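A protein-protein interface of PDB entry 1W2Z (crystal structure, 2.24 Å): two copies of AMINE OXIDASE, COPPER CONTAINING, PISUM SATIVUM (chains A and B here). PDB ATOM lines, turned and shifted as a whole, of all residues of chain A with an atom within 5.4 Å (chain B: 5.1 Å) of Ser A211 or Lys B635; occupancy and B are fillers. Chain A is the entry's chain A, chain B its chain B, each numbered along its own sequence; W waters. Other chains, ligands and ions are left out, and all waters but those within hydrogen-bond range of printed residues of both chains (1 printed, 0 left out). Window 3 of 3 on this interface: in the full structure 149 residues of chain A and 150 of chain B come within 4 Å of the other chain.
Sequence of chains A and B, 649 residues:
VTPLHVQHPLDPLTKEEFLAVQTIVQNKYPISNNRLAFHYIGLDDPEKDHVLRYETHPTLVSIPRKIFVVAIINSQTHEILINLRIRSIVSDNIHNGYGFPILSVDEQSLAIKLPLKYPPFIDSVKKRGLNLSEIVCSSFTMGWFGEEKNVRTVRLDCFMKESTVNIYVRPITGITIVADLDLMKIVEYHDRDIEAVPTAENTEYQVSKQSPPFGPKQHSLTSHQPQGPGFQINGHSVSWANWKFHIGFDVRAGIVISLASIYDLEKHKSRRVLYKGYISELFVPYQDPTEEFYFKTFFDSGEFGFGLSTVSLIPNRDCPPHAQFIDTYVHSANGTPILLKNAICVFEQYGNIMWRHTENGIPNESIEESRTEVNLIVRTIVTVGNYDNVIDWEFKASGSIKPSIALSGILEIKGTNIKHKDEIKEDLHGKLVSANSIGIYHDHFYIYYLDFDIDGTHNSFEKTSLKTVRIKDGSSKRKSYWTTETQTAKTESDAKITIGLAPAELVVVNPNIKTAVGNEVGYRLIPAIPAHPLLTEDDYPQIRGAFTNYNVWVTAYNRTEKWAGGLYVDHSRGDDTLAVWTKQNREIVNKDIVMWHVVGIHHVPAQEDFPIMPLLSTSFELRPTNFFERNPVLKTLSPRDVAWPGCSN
Ser A211 touches one residue of chain B. Of the printed residues of chain A, Lys B635 touches Ser A211, Pro A213, Phe A214 and Gly A215. Of the printed residues of chain A, Leu B265 touches Pro A213 (3.9 Å). Printed residues of chain A within 4 Å of Leu B637: Phe A214 (3.8 Å). Of the printed residues of chain A, Thr B636 touches Gly A215 and Pro A216. Pro A212 touches none of the printed residues of chain B. The nearest printed residue of chain B that does not touch Ser A211 is Leu B265 (7.9 Å). The nearest printed residue of chain A that does not touch Lys B635 is Gln A210 (4.01 Å). The nearest printed residue of chain B that does not touch Pro A213 is Thr B636 (6.7 Å).
No position is printed for both chains. Of the 10 pairs that touch across the chains among the printed residues, none has its exchanged pair printed and touching as well.
NH2 of Arg B371 sits at hydrogen-bond distance from OE1 of Gln A210 (2.9 Å). The backbone carbonyl oxygen of Leu B634 sits at hydrogen-bond distance from the side-chain amide nitrogen of Gln A210 (3.1 Å). O of Lys B635 sits at hydrogen-bond distance from N of Gly A215. O of Gly A215 sits at hydrogen-bond distance from OG1 of Thr B636 (2.7 Å).
Of the 8 printed residues of chain B, 6 touch a printed residue of chain A. Printed residues of chain B that touch a printed residue of chain A: Leu B265, Arg B371, Leu B634, Lys B635, Thr B636 and Leu B637. Printed residues of chain A that touch a printed residue of chain B: Gln A210, Ser A211, Pro A213, Phe A214, Gly A215 and Pro A216. Among the printed residues, no Asp or Glu carboxylate lies within 4 Å of a Lys or Arg side-chain nitrogen of the other chain.
Water W1 lies within hydrogen-bond range of O of Pro A216 (2.9 Å), N of Leu B637 (2.9 Å) and N of Gly A215 (3.2 Å).
Among the printed residues, pairs that only touch across the chains: Phe A214 with Lys B635 (3.3 Å), Ser A211 with Lys B635 (3.3 Å), Pro A216 with Thr B636 (3.5 Å), Phe A214 with Leu B637 (3.8 Å), Pro A213 with Leu B265 (3.9 Å) and Pro A213 with Lys B635 (3.9 Å).
The backbone carbonyl oxygen (O) of Leu B634 sits at hydrogen-bond distance from the guanidinium group (NH1) of Arg B371 (3.0 Å). O of Thr B636 is in hydrogen-bond range of NH1 of Arg B371, 3.0 Å away.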
ATOM      1  N   ASN A 202      -1.603   9.397 -19.660  1.00  0.00           N
ATOM      2  CA  ASN A 202      -1.714   9.903 -21.008  1.00  0.00           C
ATOM      3  C   ASN A 202      -2.267   8.882 -22.010  1.00  0.00           C
ATOM      4  O   ASN A 202      -1.976   9.013 -23.203  1.00  0.00           O
ATOM      5  CB  ASN A 202      -0.355  10.452 -21.504  1.00  0.00           C
ATOM      6  CG  ASN A 202      -0.001  11.844 -20.921  1.00  0.00           C
ATOM      7  OD1 ASN A 202       0.953  12.473 -21.373  1.00  0.00           O
ATOM      8  ND2 ASN A 202      -0.771  12.317 -19.945  1.00  0.00           N
ATOM      9  N   LYS A 209     -12.047  13.277 -19.592  1.00  0.00           N
ATOM     10  CA  LYS A 209     -10.973  12.762 -18.733  1.00  0.00           C
ATOM     11  C   LYS A 209      -9.583  13.278 -19.119  1.00  0.00           C
ATOM     12  O   LYS A 209      -8.580  12.774 -18.618  1.00  0.00           O
ATOM     13  CB  LYS A 209     -10.966  11.229 -18.749  1.00  0.00           C
ATOM     14  CG  LYS A 209     -12.275  10.564 -18.323  1.00  0.00           C
ATOM     15  CD  LYS A 209     -12.367  10.343 -16.831  1.00  0.00           C
ATOM     16  CE  LYS A 209     -13.788  10.000 -16.442  1.00  0.00           C
ATOM     17  NZ  LYS A 209     -14.698  11.177 -16.531  1.00  0.00           N
ATOM     18  N   GLN A 210      -9.514  14.250 -20.028  1.00  0.00           N
ATOM     19  CA  GLN A 210      -8.229  14.848 -20.398  1.00  0.00           C
ATOM     20  C   GLN A 210      -8.082  16.213 -19.716  1.00  0.00           C
ATOM     21  O   GLN A 210      -9.079  16.862 -19.375  1.00  0.00           O
ATOM     22  CB  GLN A 210      -8.144  15.014 -21.913  1.00  0.00           C
ATOM     23  CG  GLN A 210      -8.022  13.715 -22.691  1.00  0.00           C
ATOM     24  CD  GLN A 210      -7.968  13.920 -24.195  1.00  0.00           C
ATOM     25  OE1 GLN A 210      -8.547  14.875 -24.724  1.00  0.00           O
ATOM     26  NE2 GLN A 210      -7.257  13.035 -24.887  1.00  0.00           N
ATOM     27  N   SER A 211      -6.845  16.652 -19.521  1.00  0.00           N
ATOM     28  CA  SER A 211      -6.596  18.000 -18.993  1.00  0.00           C
ATOM     29  C   SER A 211      -5.911  18.905 -20.029  1.00  0.00           C
ATOM     30  O   SER A 211      -5.269  18.410 -20.958  1.00  0.00           O
ATOM     31  CB  SER A 211      -5.771  17.942 -17.688  1.00  0.00           C
ATOM     32  OG  SER A 211      -4.728  16.973 -17.743  1.00  0.00           O
ATOM     33  N   PRO A 212      -6.039  20.226 -19.868  1.00  0.00           N
ATOM     34  CA  PRO A 212      -5.340  21.185 -20.740  1.00  0.00           C
ATOM     35  C   PRO A 212      -3.810  20.981 -20.771  1.00  0.00           C
ATOM     36  O   PRO A 212      -3.265  20.270 -19.922  1.00  0.00           O
ATOM     37  CB  PRO A 212      -5.682  22.541 -20.116  1.00  0.00           C
ATOM     38  CG  PRO A 212      -6.922  22.320 -19.337  1.00  0.00           C
ATOM     39  CD  PRO A 212      -6.848  20.909 -18.839  1.00  0.00           C
ATOM     40  N   PRO A 213      -3.125  21.570 -21.750  1.00  0.00           N
ATOM     41  CA  PRO A 213      -3.738  22.398 -22.801  1.00  0.00           C
ATOM     42  C   PRO A 213      -4.335  21.595 -23.972  1.00  0.00           C
ATOM     43  O   PRO A 213      -3.885  20.490 -24.251  1.00  0.00           O
ATOM     44  CB  PRO A 213      -2.562  23.250 -23.282  1.00  0.00           C
ATOM     45  CG  PRO A 213      -1.379  22.363 -23.105  1.00  0.00           C
ATOM     46  CD  PRO A 213      -1.665  21.475 -21.914  1.00  0.00           C
ATOM     47  N   PHE A 214      -5.347  22.165 -24.620  1.00  0.00           N
ATOM     48  CA  PHE A 214      -5.932  21.625 -25.849  1.00  0.00           C
ATOM     49  C   PHE A 214      -5.573  22.517 -27.029  1.00  0.00           C
ATOM     50  O   PHE A 214      -5.219  23.697 -26.855  1.00  0.00           O
ATOM     51  CB  PHE A 214      -7.460  21.545 -25.719  1.00  0.00           C
ATOM     52  CG  PHE A 214      -7.932  20.598 -24.640  1.00  0.00           C
ATOM     53  CD1 PHE A 214      -8.097  19.238 -24.907  1.00  0.00           C
ATOM     54  CD2 PHE A 214      -8.193  21.067 -23.343  1.00  0.00           C
ATOM     55  CE1 PHE A 214      -8.531  18.354 -23.916  1.00  0.00           C
ATOM     56  CE2 PHE A 214      -8.628  20.183 -22.343  1.00  0.00           C
ATOM     57  CZ  PHE A 214      -8.798  18.823 -22.633  1.00  0.00           C
ATOM     58  N   GLY A 215      -5.674  21.952 -28.229  1.00  0.00           N
ATOM     59  CA  GLY A 215      -5.300  22.650 -29.453  1.00  0.00           C
ATOM     60  C   GLY A 215      -4.952  21.718 -30.615  1.00  0.00           C
ATOM     61  O   GLY A 215      -4.803  20.504 -30.422  1.00  0.00           O
ATOM     62  N   PRO A 216      -4.857  22.261 -31.827  1.00  0.00           N
ATOM     63  CA  PRO A 216      -5.180  23.661 -32.113  1.00  0.00           C
ATOM     64  C   PRO A 216      -6.692  23.897 -32.183  1.00  0.00           C
ATOM     65  O   PRO A 216      -7.471  22.982 -32.490  1.00  0.00           O
ATOM     66  CB  PRO A 216      -4.561  23.873 -33.482  1.00  0.00           C
ATOM     67  CG  PRO A 216      -4.736  22.533 -34.137  1.00  0.00           C
ATOM     68  CD  PRO A 216      -4.418  21.544 -33.033  1.00  0.00           C
ATOM     69  N   LEU B 265       2.628  20.655 -29.833  1.00  0.00           N
ATOM     70  CA  LEU B 265       2.113  21.199 -28.581  1.00  0.00           C
ATOM     71  C   LEU B 265       2.822  20.590 -27.376  1.00  0.00           C
ATOM     72  O   LEU B 265       3.083  21.290 -26.403  1.00  0.00           O
ATOM     73  CB  LEU B 265       0.600  20.990 -28.476  1.00  0.00           C
ATOM     74  CG  LEU B 265      -0.095  21.707 -27.315  1.00  0.00           C
ATOM     75  CD1 LEU B 265       0.037  23.236 -27.420  1.00  0.00           C
ATOM     76  CD2 LEU B 265      -1.566  21.297 -27.254  1.00  0.00           C
ATOM     77  N   ARG B 371     -14.139  12.504 -32.810  1.00  0.00           N
ATOM     78  CA  ARG B 371     -13.787  13.897 -33.061  1.00  0.00           C
ATOM     79  C   ARG B 371     -13.610  14.148 -34.526  1.00  0.00           C
ATOM     80  O   ARG B 371     -13.241  13.239 -35.270  1.00  0.00           O
ATOM     81  CB  ARG B 371     -12.494  14.252 -32.326  1.00  0.00           C
ATOM     82  CG  ARG B 371     -12.647  14.169 -30.818  1.00  0.00           C
ATOM     83  CD  ARG B 371     -11.524  14.816 -30.042  1.00  0.00           C
ATOM     84  NE  ARG B 371     -11.416  14.238 -28.712  1.00  0.00           N
ATOM     85  CZ  ARG B 371     -10.468  14.537 -27.841  1.00  0.00           C
ATOM     86  NH1 ARG B 371      -9.508  15.402 -28.146  1.00  0.00           N
ATOM     87  NH2 ARG B 371     -10.468  13.939 -26.662  1.00  0.00           N
ATOM     88  N   PRO B 632      -0.589  13.458 -32.390  1.00  0.00           N
ATOM     89  CA  PRO B 632      -0.505  14.905 -32.176  1.00  0.00           C
ATOM     90  C   PRO B 632      -1.850  15.564 -31.999  1.00  0.00           C
ATOM     91  O   PRO B 632      -1.871  16.674 -31.465  1.00  0.00           O
ATOM     92  CB  PRO B 632       0.210  15.411 -33.438  1.00  0.00           C
ATOM     93  CG  PRO B 632      -0.078  14.405 -34.474  1.00  0.00           C
ATOM     94  CD  PRO B 632      -0.103  13.085 -33.728  1.00  0.00           C
ATOM     95  N   VAL B 633      -2.939  14.925 -32.428  1.00  0.00           N
ATOM     96  CA  VAL B 633      -4.276  15.503 -32.257  1.00  0.00           C
ATOM     97  C   VAL B 633      -5.087  14.797 -31.160  1.00  0.00           C
ATOM     98  O   VAL B 633      -6.321  14.873 -31.126  1.00  0.00           O
ATOM     99  CB  VAL B 633      -5.055  15.585 -33.608  1.00  0.00           C
ATOM    100  CG1 VAL B 633      -4.349  16.581 -34.543  1.00  0.00           C
ATOM    101  CG2 VAL B 633      -5.152  14.234 -34.260  1.00  0.00           C
ATOM    102  N   LEU B 634      -4.375  14.173 -30.224  1.00  0.00           N
ATOM    103  CA  LEU B 634      -4.991  13.541 -29.070  1.00  0.00           C
ATOM    104  C   LEU B 634      -5.790  14.555 -28.277  1.00  0.00           C
ATOM    105  O   LEU B 634      -6.832  14.217 -27.725  1.00  0.00           O
ATOM    106  CB  LEU B 634      -3.916  12.918 -28.173  1.00  0.00           C
ATOM    107  CG  LEU B 634      -4.382  12.235 -26.865  1.00  0.00           C
ATOM    108  CD1 LEU B 634      -5.486  11.212 -27.111  1.00  0.00           C
ATOM    109  CD2 LEU B 634      -3.215  11.571 -26.151  1.00  0.00           C
ATOM    110  N   LYS B 635      -5.287  15.792 -28.225  1.00  0.00           N
ATOM    111  CA  LYS B 635      -5.886  16.862 -27.421  1.00  0.00           C
ATOM    112  C   LYS B 635      -6.507  17.969 -28.311  1.00  0.00           C
ATOM    113  O   LYS B 635      -6.618  19.131 -27.899  1.00  0.00           O
ATOM    114  CB  LYS B 635      -4.818  17.479 -26.513  1.00  0.00           C
ATOM    115  CG  LYS B 635      -3.958  16.474 -25.682  1.00  0.00           C
ATOM    116  CD  LYS B 635      -4.591  16.072 -24.350  1.00  0.00           C
ATOM    117  CE  LYS B 635      -3.724  16.457 -23.132  1.00  0.00           C
ATOM    118  NZ  LYS B 635      -2.762  15.387 -22.716  1.00  0.00           N
ATOM    119  N   THR B 636      -6.916  17.600 -29.523  1.00  0.00           N
ATOM    120  CA  THR B 636      -7.550  18.531 -30.442  1.00  0.00           C
ATOM    121  C   THR B 636      -9.054  18.337 -30.386  1.00  0.00           C
ATOM    122  O   THR B 636      -9.552  17.216 -30.591  1.00  0.00           O
ATOM    123  CB  THR B 636      -7.029  18.317 -31.883  1.00  0.00           C
ATOM    124  OG1 THR B 636      -5.599  18.403 -31.880  1.00  0.00           O
ATOM    125  CG2 THR B 636      -7.450  19.448 -32.793  1.00  0.00           C
ATOM    126  N   LEU B 637      -9.768  19.428 -30.096  1.00  0.00           N
ATOM    127  CA  LEU B 637     -11.208  19.390 -29.926  1.00  0.00           C
ATOM    128  C   LEU B 637     -11.875  19.659 -31.262  1.00  0.00           C
ATOM    129  O   LEU B 637     -11.384  20.452 -32.051  1.00  0.00           O
ATOM    130  CB  LEU B 637     -11.660  20.422 -28.884  1.00  0.00           C
ATOM    131  CG  LEU B 637     -11.003  20.315 -27.512  1.00  0.00           C
ATOM    132  CD1 LEU B 637     -11.371  21.506 -26.638  1.00  0.00           C
ATOM    133  CD2 LEU B 637     -11.402  18.992 -26.844  1.00  0.00           C
HETATM  134  O   HOH W   1      -8.412  22.004 -29.938  1.00  0.00           O
